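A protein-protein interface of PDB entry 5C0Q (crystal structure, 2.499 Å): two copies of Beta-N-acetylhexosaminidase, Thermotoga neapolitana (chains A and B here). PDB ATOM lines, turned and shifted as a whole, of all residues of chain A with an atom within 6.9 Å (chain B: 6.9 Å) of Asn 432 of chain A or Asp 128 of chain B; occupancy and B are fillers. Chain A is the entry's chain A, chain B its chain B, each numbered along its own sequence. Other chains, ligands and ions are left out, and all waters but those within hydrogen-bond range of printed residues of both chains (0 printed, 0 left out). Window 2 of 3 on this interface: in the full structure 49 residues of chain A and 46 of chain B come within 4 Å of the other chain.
No position is printed for both chains.
NE of Arg 431 of chain A lies within salt-bridge range of OD2 of Asp 128 of chain B (3.97 Å).
The side-chain amide nitrogen (ND2) of Asn 432 of chain A lies within hydrogen-bond range of the side-chain carboxylate (OD1) of Asp 435 of chain A, at 3.2 Å. The side-chain amide oxygen of Gln 68 of chain B sits close to the backbone NH of Leu 129 of chain B (3.2 Å). The backbone carbonyl oxygen (O) of Leu 129 of chain B is in hydrogen-bond range of the backbone NH (N) of Leu 82 of chain B, at 3.2 Å. The backbone carbonyl oxygen (O) of Ser 131 of chain B is in hydrogen-bond range of the backbone NH (N) of Leu 82 of chain B, at 3.1 Å. The backbone NH of Leu 119 of chain B sits at hydrogen-bond distance from the side-chain hydroxyl of Ser 131 of chain B (3.2 Å). OG of Ser 120 of chain B lies within hydrogen-bond range of N of Gly 123 of chain B, at 3.4 Å.
Of the 15 printed residues of chain A, 4 touch a printed residue of chain B. Hydrophobic or aromatic side chains of chain A that line the printed part of chain B: Pro 433 and Phe 434. Hydrophobic or aromatic side chains of chain B that line the printed part of chain A: Leu 82, Leu 119 and Leu 129. Among the printed residues, 8 pairs touch across the chains. Among the printed residues, Asp or Glu carboxylates within 4 Å of a Lys or Arg side-chain nitrogen of the other chain: Arg 431 of chain A with Asp 128 of chain B (3.97 Å).
Among the printed residues, pairs that only touch across the chains: Arg 431 of chain A with Gln 68 of chain B, Arg 431 of chain A with Leu 129 of chain B, Asn 432 of chain A with Asp 128 of chain B, Pro 433 of chain A with Leu 82 of chain B, Phe 434 of chain A with Leu 119 of chain B, Phe 434 of chain A with Ser 120 of chain B and Phe 434 of chain A with Glu 121 of chain B.
Val 405 of chain A touches none of the printed residues of chain B. Asn 406 of chain A touches none of the printed residues of chain B. Asn 432 of chain A touches one residue of chain B. Of the printed residues of chain A, Glu 121 of chain B touches Phe 434 (3.4 Å). Of chain A, only Arg 431 (3.4 Å) and Asn 432 (3.4 Å) come within 4 Å of Asp 128 of chain B. Printed residues of chain A within 4 Å of Leu 129 of chain B: Arg 431 (3.5 Å). The nearest residue of chain B that does not touch Asn 432 of chain A is Ser 124 of chain B (5.6 Å). The nearest printed residue of chain A that does not touch Glu 121 of chain B is Phe 438 of chain A (5.5 Å).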
ATOM      1  N   VAL A 404      23.692  12.090 -11.715  1.00  0.00           N
ATOM      2  CA  VAL A 404      23.020  12.974 -12.635  1.00  0.00           C
ATOM      3  C   VAL A 404      21.580  13.270 -12.291  1.00  0.00           C
ATOM      4  O   VAL A 404      20.737  12.394 -12.283  1.00  0.00           O
ATOM      5  CB  VAL A 404      23.029  12.395 -14.048  1.00  0.00           C
ATOM      6  CG1 VAL A 404      22.379  13.383 -14.995  1.00  0.00           C
ATOM      7  CG2 VAL A 404      24.438  12.071 -14.495  1.00  0.00           C
ATOM      8  N   VAL A 405      21.284  14.536 -12.098  1.00  0.00           N
ATOM      9  CA  VAL A 405      19.922  14.962 -11.969  1.00  0.00           C
ATOM     10  C   VAL A 405      19.629  16.130 -12.894  1.00  0.00           C
ATOM     11  O   VAL A 405      20.390  17.105 -12.947  1.00  0.00           O
ATOM     12  CB  VAL A 405      19.599  15.331 -10.533  1.00  0.00           C
ATOM     13  CG1 VAL A 405      18.309  16.097 -10.457  1.00  0.00           C
ATOM     14  CG2 VAL A 405      19.521  14.080  -9.690  1.00  0.00           C
ATOM     15  N   ASN A 406      18.575  15.974 -13.687  1.00  0.00           N
ATOM     16  CA  ASN A 406      18.062  17.033 -14.542  1.00  0.00           C
ATOM     17  C   ASN A 406      19.105  17.543 -15.536  1.00  0.00           C
ATOM     18  O   ASN A 406      19.360  18.744 -15.654  1.00  0.00           O
ATOM     19  CB  ASN A 406      17.565  18.167 -13.626  1.00  0.00           C
ATOM     20  CG  ASN A 406      16.883  19.287 -14.371  1.00  0.00           C
ATOM     21  OD1 ASN A 406      16.236  19.063 -15.402  1.00  0.00           O
ATOM     22  ND2 ASN A 406      17.047  20.510 -13.871  1.00  0.00           N
ATOM     23  N   ALA A 407      19.661  16.590 -16.275  1.00  0.00           N
ATOM     24  CA  ALA A 407      20.707  16.826 -17.251  1.00  0.00           C
ATOM     25  C   ALA A 407      20.226  17.629 -18.449  1.00  0.00           C
ATOM     26  O   ALA A 407      21.033  18.242 -19.125  1.00  0.00           O
ATOM     27  CB  ALA A 407      21.300  15.503 -17.717  1.00  0.00           C
ATOM     28  N   SER A 408      18.919  17.612 -18.702  1.00  0.00           N
ATOM     29  CA  SER A 408      18.358  18.130 -19.946  1.00  0.00           C
ATOM     30  C   SER A 408      17.753  19.515 -19.815  1.00  0.00           C
ATOM     31  O   SER A 408      17.094  19.974 -20.736  1.00  0.00           O
ATOM     32  CB  SER A 408      17.257  17.209 -20.460  1.00  0.00           C
ATOM     33  OG  SER A 408      17.633  15.858 -20.344  1.00  0.00           O
ATOM     34  N   ILE A 429      22.389   7.812 -13.616  1.00  0.00           N
ATOM     35  CA  ILE A 429      21.153   8.490 -13.925  1.00  0.00           C
ATOM     36  C   ILE A 429      20.131   8.092 -12.862  1.00  0.00           C
ATOM     37  O   ILE A 429      19.545   7.035 -12.922  1.00  0.00           O
ATOM     38  CB  ILE A 429      20.658   8.112 -15.334  1.00  0.00           C
ATOM     39  CG1 ILE A 429      21.700   8.497 -16.380  1.00  0.00           C
ATOM     40  CG2 ILE A 429      19.320   8.757 -15.646  1.00  0.00           C
ATOM     41  CD1 ILE A 429      21.776   9.963 -16.640  1.00  0.00           C
ATOM     42  N   ILE A 430      19.910   8.948 -11.891  1.00  0.00           N
ATOM     43  CA  ILE A 430      19.140   8.516 -10.766  1.00  0.00           C
ATOM     44  C   ILE A 430      17.745   9.105 -10.739  1.00  0.00           C
ATOM     45  O   ILE A 430      16.960   8.708  -9.930  1.00  0.00           O
ATOM     46  CB  ILE A 430      19.888   8.804  -9.418  1.00  0.00           C
ATOM     47  CG1 ILE A 430      20.164  10.284  -9.260  1.00  0.00           C
ATOM     48  CG2 ILE A 430      21.179   8.067  -9.373  1.00  0.00           C
ATOM     49  CD1 ILE A 430      20.699  10.652  -7.935  1.00  0.00           C
ATOM     50  N   ARG A 431      17.409  10.036 -11.622  1.00  0.00           N
ATOM     51  CA  ARG A 431      16.014  10.475 -11.628  1.00  0.00           C
ATOM     52  C   ARG A 431      15.278  10.238 -12.915  1.00  0.00           C
ATOM     53  O   ARG A 431      14.417   9.393 -12.989  1.00  0.00           O
ATOM     54  CB  ARG A 431      15.899  11.942 -11.324  1.00  0.00           C
ATOM     55  CG  ARG A 431      16.164  12.274  -9.958  1.00  0.00           C
ATOM     56  CD  ARG A 431      15.275  13.351  -9.522  1.00  0.00           C
ATOM     57  NE  ARG A 431      13.891  13.016  -9.691  1.00  0.00           N
ATOM     58  CZ  ARG A 431      12.927  13.796  -9.231  1.00  0.00           C
ATOM     59  NH1 ARG A 431      13.260  14.914  -8.611  1.00  0.00           N
ATOM     60  NH2 ARG A 431      11.650  13.477  -9.397  1.00  0.00           N
ATOM     61  N   ASN A 432      15.628  10.981 -13.943  1.00  0.00           N
ATOM     62  CA  ASN A 432      14.870  10.912 -15.166  1.00  0.00           C
ATOM     63  C   ASN A 432      15.625  10.049 -16.157  1.00  0.00           C
ATOM     64  O   ASN A 432      16.586  10.483 -16.772  1.00  0.00           O
ATOM     65  CB  ASN A 432      14.613  12.324 -15.697  1.00  0.00           C
ATOM     66  CG  ASN A 432      13.852  12.338 -17.030  1.00  0.00           C
ATOM     67  OD1 ASN A 432      13.109  11.415 -17.361  1.00  0.00           O
ATOM     68  ND2 ASN A 432      14.041  13.406 -17.794  1.00  0.00           N
ATOM     69  N   PRO A 433      15.189   8.806 -16.312  1.00  0.00           N
ATOM     70  CA  PRO A 433      15.975   7.843 -17.077  1.00  0.00           C
ATOM     71  C   PRO A 433      16.016   8.153 -18.569  1.00  0.00           C
ATOM     72  O   PRO A 433      16.720   7.468 -19.296  1.00  0.00           O
ATOM     73  CB  PRO A 433      15.258   6.523 -16.805  1.00  0.00           C
ATOM     74  CG  PRO A 433      13.863   6.924 -16.577  1.00  0.00           C
ATOM     75  CD  PRO A 433      13.907   8.250 -15.877  1.00  0.00           C
ATOM     76  N   PHE A 434      15.274   9.165 -19.005  1.00  0.00           N
ATOM     77  CA  PHE A 434      15.309   9.591 -20.396  1.00  0.00           C
ATOM     78  C   PHE A 434      16.632  10.250 -20.703  1.00  0.00           C
ATOM     79  O   PHE A 434      17.156  10.081 -21.800  1.00  0.00           O
ATOM     80  CB  PHE A 434      14.160  10.543 -20.714  1.00  0.00           C
ATOM     81  CG  PHE A 434      12.832   9.864 -20.805  1.00  0.00           C
ATOM     82  CD1 PHE A 434      12.712   8.653 -21.456  1.00  0.00           C
ATOM     83  CD2 PHE A 434      11.716  10.408 -20.206  1.00  0.00           C
ATOM     84  CE1 PHE A 434      11.505   8.024 -21.535  1.00  0.00           C
ATOM     85  CE2 PHE A 434      10.508   9.768 -20.273  1.00  0.00           C
ATOM     86  CZ  PHE A 434      10.402   8.582 -20.941  1.00  0.00           C
ATOM     87  N   ASP A 435      17.201  10.945 -19.716  1.00  0.00           N
ATOM     88  CA  ASP A 435      18.487  11.592 -19.904  1.00  0.00           C
ATOM     89  C   ASP A 435      19.553  10.663 -20.466  1.00  0.00           C
ATOM     90  O   ASP A 435      20.510  11.120 -21.040  1.00  0.00           O
ATOM     91  CB  ASP A 435      19.030  12.151 -18.589  1.00  0.00           C
ATOM     92  CG  ASP A 435      18.119  13.173 -17.939  1.00  0.00           C
ATOM     93  OD1 ASP A 435      17.175  13.662 -18.608  1.00  0.00           O
ATOM     94  OD2 ASP A 435      18.404  13.524 -16.761  1.00  0.00           O
ATOM     95  N   ALA A 436      19.384   9.356 -20.332  1.00  0.00           N
ATOM     96  CA  ALA A 436      20.444   8.439 -20.710  1.00  0.00           C
ATOM     97  C   ALA A 436      20.799   8.493 -22.193  1.00  0.00           C
ATOM     98  O   ALA A 436      21.912   8.163 -22.580  1.00  0.00           O
ATOM     99  CB  ALA A 436      20.067   7.026 -20.312  1.00  0.00           C
ATOM    100  N   PHE A 438      21.185  11.152 -23.756  1.00  0.00           N
ATOM    101  CA  PHE A 438      22.064  12.304 -23.820  1.00  0.00           C
ATOM    102  C   PHE A 438      23.516  12.019 -23.418  1.00  0.00           C
ATOM    103  O   PHE A 438      24.316  12.922 -23.320  1.00  0.00           O
ATOM    104  CB  PHE A 438      21.483  13.371 -22.916  1.00  0.00           C
ATOM    105  CG  PHE A 438      20.142  13.843 -23.354  1.00  0.00           C
ATOM    106  CD1 PHE A 438      19.720  13.631 -24.656  1.00  0.00           C
ATOM    107  CD2 PHE A 438      19.252  14.408 -22.458  1.00  0.00           C
ATOM    108  CE1 PHE A 438      18.465  14.047 -25.080  1.00  0.00           C
ATOM    109  CE2 PHE A 438      17.994  14.813 -22.880  1.00  0.00           C
ATOM    110  CZ  PHE A 438      17.602  14.631 -24.184  1.00  0.00           C
ATOM    111  N   ILE A 446      21.722   3.210 -14.818  1.00  0.00           N
ATOM    112  CA  ILE A 446      20.390   3.727 -14.547  1.00  0.00           C
ATOM    113  C   ILE A 446      19.784   3.030 -13.322  1.00  0.00           C
ATOM    114  O   ILE A 446      19.702   1.823 -13.263  1.00  0.00           O
ATOM    115  CB  ILE A 446      19.477   3.576 -15.783  1.00  0.00           C
ATOM    116  CG1 ILE A 446      20.097   4.324 -16.975  1.00  0.00           C
ATOM    117  CG2 ILE A 446      18.080   4.106 -15.520  1.00  0.00           C
ATOM    118  CD1 ILE A 446      19.450   3.978 -18.255  1.00  0.00           C
ATOM    119  N   GLN B  68       8.926   8.274  -3.995  1.00  0.00           N
ATOM    120  CA  GLN B  68       9.034   9.709  -3.842  1.00  0.00           C
ATOM    121  C   GLN B  68       8.002  10.264  -2.862  1.00  0.00           C
ATOM    122  O   GLN B  68       8.265  11.159  -2.112  1.00  0.00           O
ATOM    123  CB  GLN B  68       8.880  10.301  -5.235  1.00  0.00           C
ATOM    124  CG  GLN B  68       9.167  11.704  -5.484  1.00  0.00           C
ATOM    125  CD  GLN B  68       9.000  11.970  -6.967  1.00  0.00           C
ATOM    126  OE1 GLN B  68       9.317  11.113  -7.781  1.00  0.00           O
ATOM    127  NE2 GLN B  68       8.464  13.127  -7.322  1.00  0.00           N
ATOM    128  N   LEU B  82       8.536   3.665 -10.697  1.00  0.00           N
ATOM    129  CA  LEU B  82       9.357   3.614 -11.883  1.00  0.00           C
ATOM    130  C   LEU B  82      10.283   2.432 -11.798  1.00  0.00           C
ATOM    131  O   LEU B  82      10.442   1.705 -12.753  1.00  0.00           O
ATOM    132  CB  LEU B  82      10.142   4.898 -12.110  1.00  0.00           C
ATOM    133  CG  LEU B  82      10.855   4.844 -13.464  1.00  0.00           C
ATOM    134  CD1 LEU B  82       9.891   5.097 -14.576  1.00  0.00           C
ATOM    135  CD2 LEU B  82      11.955   5.854 -13.547  1.00  0.00           C
ATOM    136  N   LEU B 119       4.036   7.442 -17.866  1.00  0.00           N
ATOM    137  CA  LEU B 119       5.186   8.294 -17.969  1.00  0.00           C
ATOM    138  C   LEU B 119       5.315   8.784 -19.422  1.00  0.00           C
ATOM    139  O   LEU B 119       5.313   7.974 -20.341  1.00  0.00           O
ATOM    140  CB  LEU B 119       6.439   7.548 -17.548  1.00  0.00           C
ATOM    141  CG  LEU B 119       7.751   8.311 -17.658  1.00  0.00           C
ATOM    142  CD1 LEU B 119       7.801   9.432 -16.651  1.00  0.00           C
ATOM    143  CD2 LEU B 119       8.913   7.369 -17.528  1.00  0.00           C
ATOM    144  N   SER B 120       5.395  10.086 -19.638  1.00  0.00           N
ATOM    145  CA  SER B 120       5.764  10.599 -20.969  1.00  0.00           C
ATOM    146  C   SER B 120       6.968  11.485 -20.809  1.00  0.00           C
ATOM    147  O   SER B 120       7.328  11.822 -19.692  1.00  0.00           O
ATOM    148  CB  SER B 120       4.630  11.385 -21.644  1.00  0.00           C
ATOM    149  OG  SER B 120       4.385  12.609 -20.967  1.00  0.00           O
ATOM    150  N   GLU B 121       7.530  11.951 -21.914  1.00  0.00           N
ATOM    151  CA  GLU B 121       8.722  12.792 -21.837  1.00  0.00           C
ATOM    152  C   GLU B 121       8.379  14.244 -21.523  1.00  0.00           C
ATOM    153  O   GLU B 121       9.199  14.952 -20.940  1.00  0.00           O
ATOM    154  CB  GLU B 121       9.505  12.747 -23.137  1.00  0.00           C
ATOM    155  CG  GLU B 121      10.577  11.705 -23.189  1.00  0.00           C
ATOM    156  CD  GLU B 121      11.560  11.964 -24.312  1.00  0.00           C
ATOM    157  OE1 GLU B 121      11.124  12.069 -25.484  1.00  0.00           O
ATOM    158  OE2 GLU B 121      12.766  12.098 -24.014  1.00  0.00           O
ATOM    159  N   GLY B 123       5.928  15.082 -19.295  1.00  0.00           N
ATOM    160  CA  GLY B 123       5.829  15.005 -17.840  1.00  0.00           C
ATOM    161  C   GLY B 123       7.135  14.877 -17.063  1.00  0.00           C
ATOM    162  O   GLY B 123       8.073  14.200 -17.507  1.00  0.00           O
ATOM    163  N   SER B 124       7.191  15.551 -15.911  1.00  0.00           N
ATOM    164  CA  SER B 124       8.245  15.350 -14.905  1.00  0.00           C
ATOM    165  C   SER B 124       7.932  16.104 -13.608  1.00  0.00           C
ATOM    166  O   SER B 124       6.921  16.805 -13.507  1.00  0.00           O
ATOM    167  CB  SER B 124       9.596  15.800 -15.428  1.00  0.00           C
ATOM    168  OG  SER B 124       9.718  17.200 -15.292  1.00  0.00           O
ATOM    169  N   VAL B 127       6.066  13.714  -9.913  1.00  0.00           N
ATOM    170  CA  VAL B 127       5.592  13.071 -11.140  1.00  0.00           C
ATOM    171  C   VAL B 127       6.523  11.981 -11.638  1.00  0.00           C
ATOM    172  O   VAL B 127       6.109  10.925 -12.097  1.00  0.00           O
ATOM    173  CB  VAL B 127       5.455  14.075 -12.303  1.00  0.00           C
ATOM    174  CG1 VAL B 127       4.948  13.358 -13.509  1.00  0.00           C
ATOM    175  CG2 VAL B 127       4.542  15.207 -11.929  1.00  0.00           C
ATOM    176  N   ASP B 128       7.800  12.278 -11.550  1.00  0.00           N
ATOM    177  CA  ASP B 128       8.792  11.652 -12.387  1.00  0.00           C
ATOM    178  C   ASP B 128       8.990  10.186 -12.062  1.00  0.00           C
ATOM    179  O   ASP B 128       8.991   9.341 -12.928  1.00  0.00           O
ATOM    180  CB  ASP B 128      10.109  12.398 -12.232  1.00  0.00           C
ATOM    181  CG  ASP B 128      11.084  12.061 -13.315  1.00  0.00           C
ATOM    182  OD1 ASP B 128      10.721  11.239 -14.193  1.00  0.00           O
ATOM    183  OD2 ASP B 128      12.215  12.596 -13.266  1.00  0.00           O
ATOM    184  N   LEU B 129       9.158   9.892 -10.783  1.00  0.00           N
ATOM    185  CA  LEU B 129       9.362   8.542 -10.345  1.00  0.00           C
ATOM    186  C   LEU B 129       8.051   7.850  -9.933  1.00  0.00           C
ATOM    187  O   LEU B 129       8.030   6.661  -9.676  1.00  0.00           O
ATOM    188  CB  LEU B 129      10.356   8.590  -9.194  1.00  0.00           C
ATOM    189  CG  LEU B 129      11.806   8.890  -9.559  1.00  0.00           C
ATOM    190  CD1 LEU B 129      12.663   8.829  -8.366  1.00  0.00           C
ATOM    191  CD2 LEU B 129      12.321   7.903 -10.546  1.00  0.00           C
ATOM    192  N   ARG B 130       6.950   8.584  -9.921  1.00  0.00           N
ATOM    193  CA  ARG B 130       5.731   8.067  -9.371  1.00  0.00           C
ATOM    194  C   ARG B 130       4.890   7.174 -10.291  1.00  0.00           C
ATOM    195  O   ARG B 130       3.897   6.603  -9.873  1.00  0.00           O
ATOM    196  CB  ARG B 130       4.899   9.231  -8.885  1.00  0.00           C
ATOM    197  CG  ARG B 130       5.515   9.914  -7.721  1.00  0.00           C
ATOM    198  CD  ARG B 130       4.846  11.187  -7.377  1.00  0.00           C
ATOM    199  NE  ARG B 130       3.451  10.990  -7.023  1.00  0.00           N
ATOM    200  CZ  ARG B 130       2.548  11.953  -6.995  1.00  0.00           C
ATOM    201  NH1 ARG B 130       2.898  13.177  -7.280  1.00  0.00           N
ATOM    202  NH2 ARG B 130       1.312  11.702  -6.653  1.00  0.00           N
ATOM    203  N   SER B 131       5.319   7.017 -11.526  1.00  0.00           N
ATOM    204  CA  SER B 131       4.620   6.224 -12.478  1.00  0.00           C
ATOM    205  C   SER B 131       5.355   4.914 -12.765  1.00  0.00           C
ATOM    206  O   SER B 131       6.540   4.871 -12.804  1.00  0.00           O
ATOM    207  CB  SER B 131       4.406   7.064 -13.761  1.00  0.00           C
ATOM    208  OG  SER B 131       4.193   6.302 -14.921  1.00  0.00           O
